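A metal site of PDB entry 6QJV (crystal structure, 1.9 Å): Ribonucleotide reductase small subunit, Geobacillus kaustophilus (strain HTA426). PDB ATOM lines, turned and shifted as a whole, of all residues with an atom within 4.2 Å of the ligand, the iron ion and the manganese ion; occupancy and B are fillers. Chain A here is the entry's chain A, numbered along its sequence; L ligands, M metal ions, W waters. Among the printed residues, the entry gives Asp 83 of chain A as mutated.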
ATOM      1  N   LEU A  75      11.544 -32.727 -30.874  1.00  0.00           N
ATOM      2  CA  LEU A  75      12.022 -31.564 -30.140  1.00  0.00           C
ATOM      3  C   LEU A  75      10.989 -31.114 -29.113  1.00  0.00           C
ATOM      4  O   LEU A  75      11.347 -30.728 -27.998  1.00  0.00           O
ATOM      5  CB  LEU A  75      12.331 -30.433 -31.117  1.00  0.00           C
ATOM      6  CG  LEU A  75      13.221 -29.273 -30.684  1.00  0.00           C
ATOM      7  CD1 LEU A  75      14.648 -29.751 -30.370  1.00  0.00           C
ATOM      8  CD2 LEU A  75      13.222 -28.174 -31.786  1.00  0.00           C
ATOM      9  N   GLY A  78      11.194 -33.445 -26.202  1.00  0.00           N
ATOM     10  CA  GLY A  78      12.297 -33.148 -25.316  1.00  0.00           C
ATOM     11  C   GLY A  78      12.004 -31.963 -24.410  1.00  0.00           C
ATOM     12  O   GLY A  78      12.334 -31.985 -23.222  1.00  0.00           O
ATOM     13  N   PHE A  79      11.367 -30.923 -24.952  1.00  0.00           N
ATOM     14  CA  PHE A  79      11.065 -29.751 -24.152  1.00  0.00           C
ATOM     15  C   PHE A  79       9.961 -29.991 -23.148  1.00  0.00           C
ATOM     16  O   PHE A  79      10.058 -29.529 -22.015  1.00  0.00           O
ATOM     17  CB  PHE A  79      10.719 -28.563 -25.037  1.00  0.00           C
ATOM     18  CG  PHE A  79      11.896 -27.677 -25.333  1.00  0.00           C
ATOM     19  CD1 PHE A  79      12.373 -26.813 -24.357  1.00  0.00           C
ATOM     20  CD2 PHE A  79      12.535 -27.710 -26.570  1.00  0.00           C
ATOM     21  CE1 PHE A  79      13.483 -26.004 -24.608  1.00  0.00           C
ATOM     22  CE2 PHE A  79      13.642 -26.881 -26.809  1.00  0.00           C
ATOM     23  CZ  PHE A  79      14.112 -26.053 -25.824  1.00  0.00           C
ATOM     24  N   GLY A  82      11.279 -31.923 -20.403  1.00  0.00           N
ATOM     25  CA  GLY A  82      12.338 -31.177 -19.740  1.00  0.00           C
ATOM     26  C   GLY A  82      11.784 -30.069 -18.850  1.00  0.00           C
ATOM     27  O   GLY A  82      12.203 -29.902 -17.693  1.00  0.00           O
ATOM     28  N   ASP A  83      10.806 -29.318 -19.360  1.00  0.00           N
ATOM     29  CA  ASP A  83      10.194 -28.273 -18.557  1.00  0.00           C
ATOM     30  C   ASP A  83       9.409 -28.852 -17.387  1.00  0.00           C
ATOM     31  O   ASP A  83       9.403 -28.276 -16.287  1.00  0.00           O
ATOM     32  CB  ASP A  83       9.337 -27.377 -19.436  1.00  0.00           C
ATOM     33  CG  ASP A  83      10.139 -26.200 -19.984  1.00  0.00           C
ATOM     34  OD1 ASP A  83      10.704 -25.473 -19.163  1.00  0.00           O
ATOM     35  OD2 ASP A  83      10.245 -26.014 -21.202  1.00  0.00           O
ATOM     36  N   VAL A  86      12.136 -29.853 -14.729  1.00  0.00           N
ATOM     37  CA  VAL A  86      12.742 -28.740 -13.981  1.00  0.00           C
ATOM     38  C   VAL A  86      11.725 -28.019 -13.099  1.00  0.00           C
ATOM     39  O   VAL A  86      12.101 -27.451 -12.070  1.00  0.00           O
ATOM     40  CB  VAL A  86      13.479 -27.754 -14.920  1.00  0.00           C
ATOM     41  CG1 VAL A  86      14.622 -28.451 -15.627  1.00  0.00           C
ATOM     42  CG2 VAL A  86      12.575 -27.111 -15.920  1.00  0.00           C
ATOM     43  N   PHE A 112      11.639 -18.145 -10.634  1.00  0.00           N
ATOM     44  CA  PHE A 112      12.209 -19.254 -11.407  1.00  0.00           C
ATOM     45  C   PHE A 112      11.183 -20.376 -11.554  1.00  0.00           C
ATOM     46  O   PHE A 112      10.900 -20.865 -12.661  1.00  0.00           O
ATOM     47  CB  PHE A 112      13.485 -19.730 -10.682  1.00  0.00           C
ATOM     48  CG  PHE A 112      14.456 -20.560 -11.486  1.00  0.00           C
ATOM     49  CD1 PHE A 112      15.819 -20.449 -11.242  1.00  0.00           C
ATOM     50  CD2 PHE A 112      14.050 -21.509 -12.406  1.00  0.00           C
ATOM     51  CE1 PHE A 112      16.742 -21.198 -11.938  1.00  0.00           C
ATOM     52  CE2 PHE A 112      14.979 -22.288 -13.092  1.00  0.00           C
ATOM     53  CZ  PHE A 112      16.331 -22.142 -12.830  1.00  0.00           C
ATOM     54  N   GLU A 116       8.952 -21.789 -14.930  1.00  0.00           N
ATOM     55  CA  GLU A 116       8.968 -23.138 -15.486  1.00  0.00           C
ATOM     56  C   GLU A 116       7.561 -23.704 -15.569  1.00  0.00           C
ATOM     57  O   GLU A 116       7.249 -24.445 -16.495  1.00  0.00           O
ATOM     58  CB  GLU A 116       9.847 -24.054 -14.649  1.00  0.00           C
ATOM     59  CG  GLU A 116      11.349 -23.639 -14.491  1.00  0.00           C
ATOM     60  CD  GLU A 116      12.132 -23.660 -15.820  1.00  0.00           C
ATOM     61  OE1 GLU A 116      13.368 -23.499 -15.810  1.00  0.00           O
ATOM     62  OE2 GLU A 116      11.530 -23.874 -16.871  1.00  0.00           O
ATOM     63  N   HIS A 119       6.255 -22.558 -18.685  1.00  0.00           N
ATOM     64  CA  HIS A 119       6.865 -23.271 -19.809  1.00  0.00           C
ATOM     65  C   HIS A 119       6.156 -24.593 -20.070  1.00  0.00           C
ATOM     66  O   HIS A 119       5.858 -24.937 -21.221  1.00  0.00           O
ATOM     67  CB  HIS A 119       8.347 -23.508 -19.541  1.00  0.00           C
ATOM     68  CG  HIS A 119       9.129 -22.244 -19.425  1.00  0.00           C
ATOM     69  ND1 HIS A 119      10.486 -22.232 -19.171  1.00  0.00           N
ATOM     70  CD2 HIS A 119       8.741 -20.949 -19.495  1.00  0.00           C
ATOM     71  CE1 HIS A 119      10.897 -20.967 -19.111  1.00  0.00           C
ATOM     72  NE2 HIS A 119       9.851 -20.177 -19.286  1.00  0.00           N
ATOM     73  N   PHE A 149      17.493 -36.509 -17.818  1.00  0.00           N
ATOM     74  CA  PHE A 149      16.245 -35.937 -17.308  1.00  0.00           C
ATOM     75  C   PHE A 149      15.467 -36.856 -16.378  1.00  0.00           C
ATOM     76  O   PHE A 149      14.796 -36.368 -15.456  1.00  0.00           O
ATOM     77  CB  PHE A 149      15.356 -35.531 -18.485  1.00  0.00           C
ATOM     78  CG  PHE A 149      15.829 -34.264 -19.174  1.00  0.00           C
ATOM     79  CD1 PHE A 149      15.440 -33.019 -18.675  1.00  0.00           C
ATOM     80  CD2 PHE A 149      16.674 -34.316 -20.277  1.00  0.00           C
ATOM     81  CE1 PHE A 149      15.878 -31.870 -19.252  1.00  0.00           C
ATOM     82  CE2 PHE A 149      17.122 -33.138 -20.875  1.00  0.00           C
ATOM     83  CZ  PHE A 149      16.699 -31.922 -20.355  1.00  0.00           C
ATOM     84  N   VAL A 180      21.318 -28.701 -18.493  1.00  0.00           N
ATOM     85  CA  VAL A 180      19.952 -28.803 -18.980  1.00  0.00           C
ATOM     86  C   VAL A 180      19.502 -27.476 -19.623  1.00  0.00           C
ATOM     87  O   VAL A 180      18.940 -27.461 -20.729  1.00  0.00           O
ATOM     88  CB  VAL A 180      19.012 -29.245 -17.830  1.00  0.00           C
ATOM     89  CG1 VAL A 180      17.567 -28.938 -18.115  1.00  0.00           C
ATOM     90  CG2 VAL A 180      19.198 -30.733 -17.572  1.00  0.00           C
ATOM     91  N   GLU A 181      19.689 -26.359 -18.934  1.00  0.00           N
ATOM     92  CA  GLU A 181      19.294 -25.037 -19.419  1.00  0.00           C
ATOM     93  C   GLU A 181      20.369 -24.413 -20.308  1.00  0.00           C
ATOM     94  O   GLU A 181      20.087 -24.021 -21.448  1.00  0.00           O
ATOM     95  CB  GLU A 181      18.977 -24.108 -18.252  1.00  0.00           C
ATOM     96  CG  GLU A 181      17.838 -24.596 -17.334  1.00  0.00           C
ATOM     97  CD  GLU A 181      17.535 -23.673 -16.202  1.00  0.00           C
ATOM     98  OE1 GLU A 181      18.494 -23.299 -15.502  1.00  0.00           O
ATOM     99  OE2 GLU A 181      16.337 -23.308 -16.033  1.00  0.00           O
ATOM    100  N   LEU A 184      21.517 -27.556 -23.278  1.00  0.00           N
ATOM    101  CA  LEU A 184      20.462 -28.180 -24.084  1.00  0.00           C
ATOM    102  C   LEU A 184      19.321 -27.212 -24.409  1.00  0.00           C
ATOM    103  O   LEU A 184      18.918 -27.096 -25.565  1.00  0.00           O
ATOM    104  CB  LEU A 184      19.927 -29.425 -23.361  1.00  0.00           C
ATOM    105  CG  LEU A 184      20.854 -30.633 -23.326  1.00  0.00           C
ATOM    106  CD1 LEU A 184      20.255 -31.729 -22.429  1.00  0.00           C
ATOM    107  CD2 LEU A 184      21.097 -31.183 -24.687  1.00  0.00           C
ATOM    108  N   ALA A 185      18.764 -26.523 -23.405  1.00  0.00           N
ATOM    109  CA  ALA A 185      17.624 -25.643 -23.689  1.00  0.00           C
ATOM    110  C   ALA A 185      18.006 -24.542 -24.700  1.00  0.00           C
ATOM    111  O   ALA A 185      17.253 -24.250 -25.645  1.00  0.00           O
ATOM    112  CB  ALA A 185      17.103 -25.001 -22.409  1.00  0.00           C
ATOM    113  N   SER A 187      20.321 -24.507 -26.939  1.00  0.00           N
ATOM    114  CA  SER A 187      20.492 -25.078 -28.264  1.00  0.00           C
ATOM    115  C   SER A 187      19.147 -25.459 -28.859  1.00  0.00           C
ATOM    116  O   SER A 187      18.949 -25.301 -30.067  1.00  0.00           O
ATOM    117  CB  SER A 187      21.421 -26.294 -28.207  1.00  0.00           C
ATOM    118  OG  SER A 187      22.687 -25.942 -27.657  1.00  0.00           O
ATOM    119  N   GLY A 188      18.205 -25.866 -28.026  1.00  0.00           N
ATOM    120  CA  GLY A 188      16.862 -26.141 -28.510  1.00  0.00           C
ATOM    121  C   GLY A 188      16.144 -24.913 -29.032  1.00  0.00           C
ATOM    122  O   GLY A 188      15.460 -24.982 -30.067  1.00  0.00           O
ATOM    123  N   THR A 191      17.632 -24.117 -32.302  1.00  0.00           N
ATOM    124  CA  THR A 191      17.205 -25.073 -33.328  1.00  0.00           C
ATOM    125  C   THR A 191      15.806 -24.747 -33.836  1.00  0.00           C
ATOM    126  O   THR A 191      15.573 -24.707 -35.042  1.00  0.00           O
ATOM    127  CB  THR A 191      17.281 -26.496 -32.764  1.00  0.00           C
ATOM    128  OG1 THR A 191      18.638 -26.808 -32.448  1.00  0.00           O
ATOM    129  CG2 THR A 191      16.802 -27.544 -33.740  1.00  0.00           C
ATOM    130  N   GLU A 216      14.979 -17.789 -19.694  1.00  0.00           N
ATOM    131  CA  GLU A 216      16.099 -18.698 -19.495  1.00  0.00           C
ATOM    132  C   GLU A 216      17.358 -17.956 -19.148  1.00  0.00           C
ATOM    133  O   GLU A 216      18.197 -18.480 -18.415  1.00  0.00           O
ATOM    134  CB  GLU A 216      16.405 -19.528 -20.754  1.00  0.00           C
ATOM    135  CG  GLU A 216      17.158 -20.805 -20.488  1.00  0.00           C
ATOM    136  CD  GLU A 216      16.216 -21.770 -19.811  1.00  0.00           C
ATOM    137  OE1 GLU A 216      15.358 -22.325 -20.535  1.00  0.00           O
ATOM    138  OE2 GLU A 216      16.313 -21.889 -18.576  1.00  0.00           O
ATOM    139  N   HIS A 219      17.531 -17.809 -15.467  1.00  0.00           N
ATOM    140  CA  HIS A 219      17.813 -19.123 -14.898  1.00  0.00           C
ATOM    141  C   HIS A 219      19.300 -19.445 -14.972  1.00  0.00           C
ATOM    142  O   HIS A 219      19.915 -19.922 -13.997  1.00  0.00           O
ATOM    143  CB  HIS A 219      16.972 -20.196 -15.625  1.00  0.00           C
ATOM    144  CG  HIS A 219      15.503 -19.912 -15.634  1.00  0.00           C
ATOM    145  ND1 HIS A 219      14.588 -20.709 -16.294  1.00  0.00           N
ATOM    146  CD2 HIS A 219      14.792 -18.902 -15.075  1.00  0.00           C
ATOM    147  CE1 HIS A 219      13.373 -20.202 -16.118  1.00  0.00           C
ATOM    148  NE2 HIS A 219      13.476 -19.097 -15.391  1.00  0.00           N
ATOM    149  N   TYR A 255      22.312 -37.549 -27.018  1.00  0.00           N
ATOM    150  CA  TYR A 255      20.962 -37.123 -27.361  1.00  0.00           C
ATOM    151  C   TYR A 255      20.980 -36.283 -28.635  1.00  0.00           C
ATOM    152  O   TYR A 255      20.116 -36.445 -29.503  1.00  0.00           O
ATOM    153  CB  TYR A 255      20.348 -36.377 -26.189  1.00  0.00           C
ATOM    154  CG  TYR A 255      18.970 -35.812 -26.450  1.00  0.00           C
ATOM    155  CD1 TYR A 255      17.915 -36.642 -26.811  1.00  0.00           C
ATOM    156  CD2 TYR A 255      18.720 -34.460 -26.308  1.00  0.00           C
ATOM    157  CE1 TYR A 255      16.623 -36.099 -27.029  1.00  0.00           C
ATOM    158  CE2 TYR A 255      17.432 -33.923 -26.537  1.00  0.00           C
ATOM    159  CZ  TYR A 255      16.401 -34.755 -26.880  1.00  0.00           C
ATOM    160  OH  TYR A 255      15.131 -34.193 -27.085  1.00  0.00           O
ATOM    161  N   VAL A 256      21.948 -35.368 -28.775  1.00  0.00           N
ATOM    162  CA  VAL A 256      21.991 -34.515 -29.954  1.00  0.00           C
ATOM    163  C   VAL A 256      22.156 -35.380 -31.211  1.00  0.00           C
ATOM    164  O   VAL A 256      21.434 -35.209 -32.197  1.00  0.00           O
ATOM    165  CB  VAL A 256      23.100 -33.460 -29.826  1.00  0.00           C
ATOM    166  CG1 VAL A 256      23.352 -32.729 -31.160  1.00  0.00           C
ATOM    167  CG2 VAL A 256      22.776 -32.439 -28.764  1.00  0.00           C
ATOM    168  N   LEU A 259      18.782 -37.063 -32.080  1.00  0.00           N
ATOM    169  CA  LEU A 259      17.856 -36.155 -32.753  1.00  0.00           C
ATOM    170  C   LEU A 259      18.324 -35.856 -34.168  1.00  0.00           C
ATOM    171  O   LEU A 259      17.519 -35.656 -35.081  1.00  0.00           O
ATOM    172  CB  LEU A 259      17.740 -34.842 -32.000  1.00  0.00           C
ATOM    173  CG  LEU A 259      17.077 -34.922 -30.631  1.00  0.00           C
ATOM    174  CD1 LEU A 259      17.082 -33.539 -30.060  1.00  0.00           C
ATOM    175  CD2 LEU A 259      15.652 -35.450 -30.741  1.00  0.00           C
ATOM    176  N   LEU A 282      24.165 -27.158 -36.215  1.00  0.00           N
ATOM    177  CA  LEU A 282      23.483 -27.282 -34.931  1.00  0.00           C
ATOM    178  C   LEU A 282      24.379 -27.989 -33.924  1.00  0.00           C
ATOM    179  O   LEU A 282      24.453 -27.599 -32.751  1.00  0.00           O
ATOM    180  CB  LEU A 282      22.163 -28.025 -35.096  1.00  0.00           C
ATOM    181  CG  LEU A 282      21.114 -27.372 -36.009  1.00  0.00           C
ATOM    182  CD1 LEU A 282      19.925 -28.303 -36.226  1.00  0.00           C
ATOM    183  CD2 LEU A 282      20.644 -26.019 -35.471  1.00  0.00           C
HETATM  184  C1  LIG L   1      14.174 -25.457 -18.722  1.00  0.00           C
HETATM  185  O1  LIG L   1      14.872 -24.706 -17.934  1.00  0.00           O
HETATM  186  O2  LIG L   1      12.984 -25.315 -19.070  1.00  0.00           O
HETATM  187  C2  LIG L   1      14.899 -26.729 -19.290  1.00  0.00           C
HETATM  188  C3  LIG L   1      14.353 -27.285 -20.580  1.00  0.00           C
HETATM  189  C4  LIG L   1      15.085 -28.470 -21.085  1.00  0.00           C
HETATM  190  C5  LIG L   1      14.815 -28.746 -22.544  1.00  0.00           C
HETATM  191  C6  LIG L   1      15.395 -30.046 -23.004  1.00  0.00           C
HETATM  192  C7  LIG L   1      15.081 -30.377 -24.456  1.00  0.00           C
HETATM  193  C8  LIG L   1      15.815 -29.500 -25.362  1.00  0.00           C
HETATM  194  C9  LIG L   1      16.087 -30.095 -26.712  1.00  0.00           C
HETATM  195  C10 LIG L   1      17.590 -30.097 -27.043  1.00  0.00           C
HETATM  196  C11 LIG L   1      17.838 -29.862 -28.483  1.00  0.00           C
HETATM  197  C12 LIG L   1      19.318 -29.768 -28.849  1.00  0.00           C
HETATM  198  C13 LIG L   1      19.516 -29.520 -30.349  1.00  0.00           C
HETATM  199  C14 LIG L   1      19.799 -30.760 -31.177  1.00  0.00           C
HETATM  200  C15 LIG L   1      19.950 -30.494 -32.694  1.00  0.00           C
HETATM  201  C16 LIG L   1      18.931 -31.270 -33.589  1.00  0.00           C
HETATM  202 FE    FE M   1      14.787 -22.763 -17.182  1.00  0.00          FE
HETATM  203 MN    MN M   2      11.951 -23.856 -18.960  1.00  0.00          MN
HETATM  204  O   HOH W   1      12.113 -24.068 -21.224  1.00  0.00           O
HETATM  205  O   HOH W   2      13.599 -22.596 -18.721  1.00  0.00           O
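Merely in contact with the ligand: Gly 78 (3.4 Å), Phe 149 (3.5 Å), Thr 191 (3.5 Å), Leu 184 (3.6 Å), Phe 79 (3.6 Å), Val 86 (3.6 Å), Val 180 (3.7 Å), Leu 75 (3.7 Å), Gly 188 (3.8 Å) and Tyr 255 (3.9 Å). Hydrophobic or aromatic side chains within 4 Å of the ligand: Leu 75, Phe 79, Val 86, Phe 149, Val 180 and Tyr 255. Within 4 Å of the ligand: Leu 75, Gly 78, Phe 79, Asp 83, Val 86, Glu 116, His 119, Phe 149, Val 180, Glu 181, Leu 184, Gly 188, Thr 191, Glu 216 and Tyr 255. The nearest printed residue that does not touch the ligand is Ala 185 (4.02 Å).
The iron ion is bound by water W2, the side-chain carboxylate (OE2) of Glu 181, an oxygen (O1) of the ligand, the side-chain carboxylate (OE1) of Glu 116, the side-chain carboxylate (OE2) of Glu 216 and a ring nitrogen (ND1) of His 219. The iron ion has six donor atoms within binding distance.
O of Val 180 is in hydrogen-bond range of N of Ala 185 (2.8 Å). The backbone carbonyl oxygen of Ser 187 sits at hydrogen-bond distance from the side-chain hydroxyl of Thr 191 (2.8 Å).
The manganese ion is bound by an oxygen (O2) of the ligand (1.8 Å), the side-chain carboxylate (OD1) of Asp 83 (2.1 Å), water W2 (2.1 Å), the side-chain carboxylate (OE2) of Glu 116 (2.1 Å), a ring nitrogen (ND1) of His 119 (2.2 Å) and water W1 (2.3 Å).
Four residues have an atom within 4 Å of the iron ion: Glu 116, Glu 181, Glu 216 and His 219.
Along chain A the residues within 4 Å of the manganese ion span positions 83 to 119.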
